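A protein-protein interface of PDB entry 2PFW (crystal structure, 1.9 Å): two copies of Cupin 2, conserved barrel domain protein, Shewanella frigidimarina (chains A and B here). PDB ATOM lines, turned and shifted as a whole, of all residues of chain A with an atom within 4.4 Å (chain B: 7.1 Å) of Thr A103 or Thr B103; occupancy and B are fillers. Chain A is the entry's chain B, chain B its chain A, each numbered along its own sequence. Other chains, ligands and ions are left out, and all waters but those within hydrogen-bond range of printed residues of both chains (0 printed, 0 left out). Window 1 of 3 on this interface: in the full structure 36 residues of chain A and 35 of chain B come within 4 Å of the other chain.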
ATOM      1  N   LEU A  34       9.122   9.997   0.138  1.00  0.00           N
ATOM      2  CA  LEU A  34       8.806  10.238  -1.266  1.00  0.00           C
ATOM      3  C   LEU A  34       7.627   9.369  -1.691  1.00  0.00           C
ATOM      4  O   LEU A  34       7.502   8.221  -1.263  1.00  0.00           O
ATOM      5  CB  LEU A  34      10.007   9.972  -2.166  1.00  0.00           C
ATOM      6  CG  LEU A  34       9.782   9.906  -3.676  1.00  0.00           C
ATOM      7  CD1 LEU A  34       9.106  11.161  -4.203  1.00  0.00           C
ATOM      8  CD2 LEU A  34      11.104   9.689  -4.407  1.00  0.00           C
ATOM      9  N   MET A  35       6.752   9.915  -2.539  1.00  0.00           N
ATOM     10  CA  MET A  35       5.582   9.138  -2.956  1.00  0.00           C
ATOM     11  C   MET A  35       5.052   9.554  -4.319  1.00  0.00           C
ATOM     12  O   MET A  35       4.981  10.718  -4.563  1.00  0.00           O
ATOM     13  CB  MET A  35       4.473   9.230  -1.897  1.00  0.00           C
ATOM     14  CG  MET A  35       3.227   8.428  -2.287  1.00  0.00           C
ATOM     15  SD  MET A  35       1.795   8.379  -0.949  1.00  0.00           S
ATOM     16  CE  MET A  35       2.274   6.730  -0.211  1.00  0.00           C
ATOM     17  N   ALA A  36       4.714   8.575  -5.156  1.00  0.00           N
ATOM     18  CA  ALA A  36       4.189   8.889  -6.487  1.00  0.00           C
ATOM     19  C   ALA A  36       2.937   8.057  -6.745  1.00  0.00           C
ATOM     20  O   ALA A  36       2.966   6.834  -6.603  1.00  0.00           O
ATOM     21  CB  ALA A  36       5.218   8.660  -7.576  1.00  0.00           C
ATOM     22  N   SER A  55       5.215  18.754   0.240  1.00  0.00           N
ATOM     23  CA  SER A  55       5.504  19.347  -1.067  1.00  0.00           C
ATOM     24  C   SER A  55       4.791  18.524  -2.139  1.00  0.00           C
ATOM     25  O   SER A  55       4.544  17.333  -1.941  1.00  0.00           O
ATOM     26  CB  SER A  55       7.001  19.413  -1.315  1.00  0.00           C
ATOM     27  OG  SER A  55       7.608  20.497  -0.638  1.00  0.00           O
ATOM     28  N   GLN A  56       4.437  19.143  -3.259  1.00  0.00           N
ATOM     29  CA  GLN A  56       3.752  18.384  -4.309  1.00  0.00           C
ATOM     30  C   GLN A  56       4.293  18.779  -5.682  1.00  0.00           C
ATOM     31  O   GLN A  56       4.399  19.965  -6.004  1.00  0.00           O
ATOM     32  CB  GLN A  56       2.235  18.577  -4.266  1.00  0.00           C
ATOM     33  CG  GLN A  56       1.494  17.806  -5.348  1.00  0.00           C
ATOM     34  CD  GLN A  56      -0.013  17.854  -5.245  1.00  0.00           C
ATOM     35  OE1 GLN A  56      -0.593  18.020  -4.174  1.00  0.00           O
ATOM     36  NE2 GLN A  56      -0.686  17.700  -6.385  1.00  0.00           N
ATOM     37  N   VAL A  57       4.660  17.788  -6.498  1.00  0.00           N
ATOM     38  CA  VAL A  57       4.932  18.082  -7.912  1.00  0.00           C
ATOM     39  C   VAL A  57       4.078  17.130  -8.753  1.00  0.00           C
ATOM     40  O   VAL A  57       3.976  15.940  -8.469  1.00  0.00           O
ATOM     41  CB  VAL A  57       6.408  18.000  -8.283  1.00  0.00           C
ATOM     42  CG1 VAL A  57       6.643  18.418  -9.730  1.00  0.00           C
ATOM     43  CG2 VAL A  57       7.238  18.892  -7.368  1.00  0.00           C
ATOM     44  N   ILE A 101      -0.165  12.316 -12.632  1.00  0.00           N
ATOM     45  CA  ILE A 101       0.742  11.755 -11.629  1.00  0.00           C
ATOM     46  C   ILE A 101       1.027  12.811 -10.565  1.00  0.00           C
ATOM     47  O   ILE A 101       1.494  13.903 -10.883  1.00  0.00           O
ATOM     48  CB  ILE A 101       2.025  11.257 -12.299  1.00  0.00           C
ATOM     49  CG1 ILE A 101       1.718  10.054 -13.205  1.00  0.00           C
ATOM     50  CG2 ILE A 101       3.119  10.936 -11.300  1.00  0.00           C
ATOM     51  CD1 ILE A 101       2.901   9.644 -14.038  1.00  0.00           C
ATOM     52  N   ASP A 102       0.732  12.471  -9.316  1.00  0.00           N
ATOM     53  CA  ASP A 102       0.972  13.347  -8.178  1.00  0.00           C
ATOM     54  C   ASP A 102       2.154  12.820  -7.364  1.00  0.00           C
ATOM     55  O   ASP A 102       2.119  11.656  -6.961  1.00  0.00           O
ATOM     56  CB  ASP A 102      -0.266  13.422  -7.289  1.00  0.00           C
ATOM     57  CG  ASP A 102      -1.347  14.362  -7.772  1.00  0.00           C
ATOM     58  OD1 ASP A 102      -1.051  15.328  -8.504  1.00  0.00           O
ATOM     59  OD2 ASP A 102      -2.518  14.146  -7.402  1.00  0.00           O
ATOM     60  N   THR A 103       3.155  13.652  -7.137  1.00  0.00           N
ATOM     61  CA  THR A 103       4.298  13.248  -6.321  1.00  0.00           C
ATOM     62  C   THR A 103       4.442  14.130  -5.089  1.00  0.00           C
ATOM     63  O   THR A 103       4.319  15.350  -5.198  1.00  0.00           O
ATOM     64  CB  THR A 103       5.592  13.307  -7.143  1.00  0.00           C
ATOM     65  OG1 THR A 103       6.040  14.657  -7.289  1.00  0.00           O
ATOM     66  CG2 THR A 103       5.309  12.810  -8.557  1.00  0.00           C
ATOM     67  N   PHE A 104       4.695  13.506  -3.948  1.00  0.00           N
ATOM     68  CA  PHE A 104       4.723  14.167  -2.651  1.00  0.00           C
ATOM     69  C   PHE A 104       6.033  13.930  -1.907  1.00  0.00           C
ATOM     70  O   PHE A 104       6.483  12.780  -1.860  1.00  0.00           O
ATOM     71  CB  PHE A 104       3.583  13.655  -1.761  1.00  0.00           C
ATOM     72  CG  PHE A 104       2.202  13.873  -2.351  1.00  0.00           C
ATOM     73  CD1 PHE A 104       1.578  15.101  -2.221  1.00  0.00           C
ATOM     74  CD2 PHE A 104       1.554  12.849  -3.020  1.00  0.00           C
ATOM     75  CE1 PHE A 104       0.319  15.310  -2.757  1.00  0.00           C
ATOM     76  CE2 PHE A 104       0.298  13.048  -3.560  1.00  0.00           C
ATOM     77  CZ  PHE A 104      -0.316  14.283  -3.429  1.00  0.00           C
ATOM     78  N   LEU B  28      10.231  19.396 -14.371  1.00  0.00           N
ATOM     79  CA  LEU B  28       8.782  19.486 -14.238  1.00  0.00           C
ATOM     80  C   LEU B  28       8.379  20.338 -13.036  1.00  0.00           C
ATOM     81  O   LEU B  28       7.341  21.001 -13.044  1.00  0.00           O
ATOM     82  CB  LEU B  28       8.167  18.096 -14.089  1.00  0.00           C
ATOM     83  CG  LEU B  28       8.472  17.127 -15.241  1.00  0.00           C
ATOM     84  CD1 LEU B  28       7.820  15.783 -14.990  1.00  0.00           C
ATOM     85  CD2 LEU B  28       8.020  17.726 -16.562  1.00  0.00           C
ATOM     86  N   GLY B  29       9.196  20.310 -11.989  1.00  0.00           N
ATOM     87  CA  GLY B  29       8.962  21.155 -10.823  1.00  0.00           C
ATOM     88  C   GLY B  29       9.811  20.699  -9.650  1.00  0.00           C
ATOM     89  O   GLY B  29      10.068  19.502  -9.511  1.00  0.00           O
ATOM     90  N   LEU B  34      11.787  18.143  -2.897  1.00  0.00           N
ATOM     91  CA  LEU B  34      11.047  17.340  -3.873  1.00  0.00           C
ATOM     92  C   LEU B  34      11.365  17.811  -5.282  1.00  0.00           C
ATOM     93  O   LEU B  34      11.511  19.012  -5.511  1.00  0.00           O
ATOM     94  CB  LEU B  34       9.539  17.404  -3.633  1.00  0.00           C
ATOM     95  CG  LEU B  34       8.669  16.578  -4.584  1.00  0.00           C
ATOM     96  CD1 LEU B  34       8.919  15.088  -4.397  1.00  0.00           C
ATOM     97  CD2 LEU B  34       7.191  16.882  -4.382  1.00  0.00           C
ATOM     98  N   MET B  35      11.493  16.887  -6.232  1.00  0.00           N
ATOM     99  CA  MET B  35      11.912  17.282  -7.581  1.00  0.00           C
ATOM    100  C   MET B  35      11.532  16.243  -8.631  1.00  0.00           C
ATOM    101  O   MET B  35      11.776  15.101  -8.410  1.00  0.00           O
ATOM    102  CB  MET B  35      13.416  17.562  -7.629  1.00  0.00           C
ATOM    103  CG  MET B  35      14.018  17.635  -9.030  1.00  0.00           C
ATOM    104  SD  MET B  35      15.916  18.094  -9.116  1.00  0.00           S
ATOM    105  CE  MET B  35      15.702  19.933  -9.329  1.00  0.00           C
ATOM    106  N   ALA B  36      10.945  16.705  -9.730  1.00  0.00           N
ATOM    107  CA  ALA B  36      10.501  15.816 -10.798  1.00  0.00           C
ATOM    108  C   ALA B  36      11.032  16.308 -12.140  1.00  0.00           C
ATOM    109  O   ALA B  36      10.889  17.484 -12.484  1.00  0.00           O
ATOM    110  CB  ALA B  36       8.989  15.721 -10.820  1.00  0.00           C
ATOM    111  N   VAL B  37      11.656  15.409 -12.900  1.00  0.00           N
ATOM    112  CA  VAL B  37      12.137  15.774 -14.229  1.00  0.00           C
ATOM    113  C   VAL B  37      11.588  14.780 -15.264  1.00  0.00           C
ATOM    114  O   VAL B  37      11.102  13.716 -14.884  1.00  0.00           O
ATOM    115  CB  VAL B  37      13.668  15.813 -14.340  1.00  0.00           C
ATOM    116  CG1 VAL B  37      14.251  16.765 -13.308  1.00  0.00           C
ATOM    117  CG2 VAL B  37      14.249  14.413 -14.190  1.00  0.00           C
ATOM    118  N   HIS B  54      19.507  10.259  -2.430  1.00  0.00           N
ATOM    119  CA  HIS B  54      18.135  10.664  -2.710  1.00  0.00           C
ATOM    120  C   HIS B  54      17.198   9.477  -2.869  1.00  0.00           C
ATOM    121  O   HIS B  54      17.533   8.482  -3.525  1.00  0.00           O
ATOM    122  CB  HIS B  54      18.096  11.515  -3.982  1.00  0.00           C
ATOM    123  CG  HIS B  54      19.043  12.667  -4.002  1.00  0.00           C
ATOM    124  ND1 HIS B  54      20.389  12.531  -4.260  1.00  0.00           N
ATOM    125  CD2 HIS B  54      18.839  13.993  -3.801  1.00  0.00           C
ATOM    126  CE1 HIS B  54      20.977  13.713  -4.216  1.00  0.00           C
ATOM    127  NE2 HIS B  54      20.053  14.619  -3.937  1.00  0.00           N
ATOM    128  N   SER B  55      16.001   9.540  -2.276  1.00  0.00           N
ATOM    129  CA  SER B  55      14.971   8.561  -2.627  1.00  0.00           C
ATOM    130  C   SER B  55      14.537   8.830  -4.068  1.00  0.00           C
ATOM    131  O   SER B  55      14.651   9.955  -4.554  1.00  0.00           O
ATOM    132  CB  SER B  55      13.797   8.611  -1.664  1.00  0.00           C
ATOM    133  OG  SER B  55      14.047   7.828  -0.512  1.00  0.00           O
ATOM    134  N   GLN B  56      14.066   7.803  -4.765  1.00  0.00           N
ATOM    135  CA  GLN B  56      13.718   7.990  -6.175  1.00  0.00           C
ATOM    136  C   GLN B  56      12.502   7.135  -6.523  1.00  0.00           C
ATOM    137  O   GLN B  56      12.470   5.939  -6.226  1.00  0.00           O
ATOM    138  CB  GLN B  56      14.888   7.658  -7.099  1.00  0.00           C
ATOM    139  CG  GLN B  56      14.570   7.773  -8.583  1.00  0.00           C
ATOM    140  CD  GLN B  56      15.692   7.284  -9.476  1.00  0.00           C
ATOM    141  OE1 GLN B  56      16.879   7.436  -9.189  1.00  0.00           O
ATOM    142  NE2 GLN B  56      15.321   6.681 -10.599  1.00  0.00           N
ATOM    143  N   VAL B  57      11.505   7.759  -7.148  1.00  0.00           N
ATOM    144  CA  VAL B  57      10.404   6.995  -7.751  1.00  0.00           C
ATOM    145  C   VAL B  57      10.354   7.351  -9.234  1.00  0.00           C
ATOM    146  O   VAL B  57      10.514   8.518  -9.594  1.00  0.00           O
ATOM    147  CB  VAL B  57       9.070   7.244  -7.052  1.00  0.00           C
ATOM    148  CG1 VAL B  57       7.982   6.299  -7.545  1.00  0.00           C
ATOM    149  CG2 VAL B  57       9.215   7.071  -5.542  1.00  0.00           C
ATOM    150  N   SER B  58      10.174   6.344 -10.085  1.00  0.00           N
ATOM    151  CA  SER B  58      10.251   6.552 -11.528  1.00  0.00           C
ATOM    152  C   SER B  58       9.018   5.944 -12.199  1.00  0.00           C
ATOM    153  O   SER B  58       8.537   4.884 -11.805  1.00  0.00           O
ATOM    154  CB  SER B  58      11.531   5.952 -12.099  1.00  0.00           C
ATOM    155  OG  SER B  58      12.596   6.868 -12.179  1.00  0.00           O
ATOM    156  N   TYR B  59       8.518   6.651 -13.208  1.00  0.00           N
ATOM    157  CA  TYR B  59       7.347   6.235 -13.966  1.00  0.00           C
ATOM    158  C   TYR B  59       7.698   6.119 -15.449  1.00  0.00           C
ATOM    159  O   TYR B  59       8.361   7.005 -15.986  1.00  0.00           O
ATOM    160  CB  TYR B  59       6.182   7.215 -13.790  1.00  0.00           C
ATOM    161  CG  TYR B  59       4.951   6.794 -14.572  1.00  0.00           C
ATOM    162  CD1 TYR B  59       4.126   5.783 -14.124  1.00  0.00           C
ATOM    163  CD2 TYR B  59       4.626   7.429 -15.769  1.00  0.00           C
ATOM    164  CE1 TYR B  59       3.000   5.398 -14.835  1.00  0.00           C
ATOM    165  CE2 TYR B  59       3.506   7.049 -16.484  1.00  0.00           C
ATOM    166  CZ  TYR B  59       2.704   6.040 -16.015  1.00  0.00           C
ATOM    167  OH  TYR B  59       1.589   5.667 -16.738  1.00  0.00           O
ATOM    168  N   ILE B 101       9.574   9.629 -16.156  1.00  0.00           N
ATOM    169  CA  ILE B 101       9.486  10.676 -15.137  1.00  0.00           C
ATOM    170  C   ILE B 101      10.265  10.241 -13.899  1.00  0.00           C
ATOM    171  O   ILE B 101       9.870   9.293 -13.230  1.00  0.00           O
ATOM    172  CB  ILE B 101       8.019  10.998 -14.786  1.00  0.00           C
ATOM    173  CG1 ILE B 101       7.105  11.193 -15.993  1.00  0.00           C
ATOM    174  CG2 ILE B 101       7.985  12.180 -13.824  1.00  0.00           C
ATOM    175  CD1 ILE B 101       6.650  12.572 -16.385  1.00  0.00           C
ATOM    176  N   ASP B 102      11.374  10.911 -13.632  1.00  0.00           N
ATOM    177  CA  ASP B 102      12.180  10.632 -12.447  1.00  0.00           C
ATOM    178  C   ASP B 102      11.846  11.661 -11.361  1.00  0.00           C
ATOM    179  O   ASP B 102      11.992  12.851 -11.635  1.00  0.00           O
ATOM    180  CB  ASP B 102      13.670  10.682 -12.749  1.00  0.00           C
ATOM    181  CG  ASP B 102      14.241   9.505 -13.508  1.00  0.00           C
ATOM    182  OD1 ASP B 102      13.653   8.407 -13.514  1.00  0.00           O
ATOM    183  OD2 ASP B 102      15.317   9.667 -14.123  1.00  0.00           O
ATOM    184  N   THR B 103      11.428  11.187 -10.198  1.00  0.00           N
ATOM    185  CA  THR B 103      11.228  12.051  -9.042  1.00  0.00           C
ATOM    186  C   THR B 103      12.107  11.626  -7.869  1.00  0.00           C
ATOM    187  O   THR B 103      12.266  10.431  -7.625  1.00  0.00           O
ATOM    188  CB  THR B 103       9.755  12.044  -8.599  1.00  0.00           C
ATOM    189  OG1 THR B 103       9.490  10.930  -7.749  1.00  0.00           O
ATOM    190  CG2 THR B 103       8.863  11.874  -9.829  1.00  0.00           C
ATOM    191  N   PHE B 104      12.652  12.610  -7.171  1.00  0.00           N
ATOM    192  CA  PHE B 104      13.609  12.418  -6.094  1.00  0.00           C
ATOM    193  C   PHE B 104      13.212  13.157  -4.819  1.00  0.00           C
ATOM    194  O   PHE B 104      12.797  14.316  -4.908  1.00  0.00           O
ATOM    195  CB  PHE B 104      14.989  12.929  -6.527  1.00  0.00           C
ATOM    196  CG  PHE B 104      15.461  12.293  -7.824  1.00  0.00           C
ATOM    197  CD1 PHE B 104      16.060  11.044  -7.802  1.00  0.00           C
ATOM    198  CD2 PHE B 104      15.287  12.953  -9.028  1.00  0.00           C
ATOM    199  CE1 PHE B 104      16.485  10.449  -8.975  1.00  0.00           C
ATOM    200  CE2 PHE B 104      15.720  12.363 -10.198  1.00  0.00           C
ATOM    201  CZ  PHE B 104      16.316  11.115 -10.171  1.00  0.00           C
ATOM    202  N   SER B 105      13.347  12.536  -3.650  1.00  0.00           N
ATOM    203  CA  SER B 105      13.305  13.310  -2.413  1.00  0.00           C
ATOM    204  C   SER B 105      14.702  13.396  -1.766  1.00  0.00           C
ATOM    205  O   SER B 105      15.135  12.210  -1.566  1.00  0.00           O
ATOM    206  CB  SER B 105      12.336  12.784  -1.359  1.00  0.00           C
ATOM    207  OG  SER B 105      12.271  13.760  -0.316  1.00  0.00           O
ATOM    208  N   PRO B 106      15.575  14.291  -1.317  1.00  0.00           N
ATOM    209  CA  PRO B 106      15.962  15.718  -1.391  1.00  0.00           C
ATOM    210  C   PRO B 106      15.886  16.095  -2.872  1.00  0.00           C
ATOM    211  O   PRO B 106      15.795  15.181  -3.700  1.00  0.00           O
ATOM    212  CB  PRO B 106      17.381  15.820  -0.870  1.00  0.00           C
ATOM    213  CG  PRO B 106      17.828  14.408  -0.715  1.00  0.00           C
ATOM    214  CD  PRO B 106      16.580  13.658  -0.368  1.00  0.00           C
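N of Leu B28 lies within hydrogen-bond range of O of Ala B36 (2.8 Å). The backbone NH of Ala B36 is in hydrogen-bond range of the backbone carbonyl oxygen of Gly B29, 2.9 Å away. The backbone NH of Val B57 sits at hydrogen-bond distance from the backbone carbonyl oxygen of Thr B103, 2.8 Å away. N of Phe A104 is in hydrogen-bond range of O of Met A35, 2.9 Å away. The side-chain carboxylate (OD1) of Asp A102 sits at hydrogen-bond distance from the side-chain amide nitrogen (NE2) of Gln A56, 3.2 Å away. The backbone carbonyl oxygen of Val A57 sits at hydrogen-bond distance from the side-chain hydroxyl of Thr A103, 2.7 Å away.
Among the printed residues, pairs that only touch across the chains: Leu A34 with Leu B34 (3.9 Å), Leu A34 with Ser B55 (3.6 Å), Leu A34 with Gln B56 (3.5 Å), Leu A34 with Val B57 (3.4 Å), Leu A34 with Thr B103 (3.5 Å), Leu A34 with Ser B105 (3.7 Å), Ala A36 with Val B57 (3.6 Å), Ser A55 with Leu B34 (3.6 Å), Gln A56 with Leu B34 (3.7 Å), Val A57 with Gly B29 (3.6 Å), Val A57 with Leu B34 (3.4 Å), Val A57 with Ala B36 (3.7 Å), Ile A101 with Tyr B59 (3.3 Å), Thr A103 with Leu B34 (3.4 Å), Thr A103 with Thr B103 (3.9 Å) and Phe A104 with Leu B34 (3.98 Å).
Of the printed residues of chain B, Thr A103 touches Leu B34 and Thr B103. Of chain A, only Leu A34 (3.5 Å) and Thr A103 (3.9 Å) come within 4 Å of Thr B103. Printed residues of chain B within 4 Å of Phe A104: Leu B34 (3.98 Å). Of the printed residues of chain A, Gly B29 touches Val A57. His B54 touches none of the printed residues of chain A. Ile B101 touches none of the printed residues of chain A. The nearest residue of chain B that does not touch Thr A103 is Ala B36 (4.7 Å). The nearest printed residue of chain B that does not touch Ala A36 is Thr B103 (4.8 Å).
Hydrophobic or aromatic side chains of chain B within 4 Å of the printed part of chain A: Leu B34, Ala B36, Val B57 and Tyr B59. Among the printed residues, 16 pairs touch across the chains.
Leu A34 touches its own counterpart, Leu B34. Leu A34 touches Gln B56, and with the chains exchanged Gln A56 touches Leu B34. Leu A34 touches Thr B103, and with the chains exchanged Thr A103 touches Leu B34. Ala A36 touches Val B57, and with the chains exchanged Val A57 touches Ala B36. Positions printed for both chains: 34, 35, 36, 55, 56, 57, 101, 102, 103 and 104.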
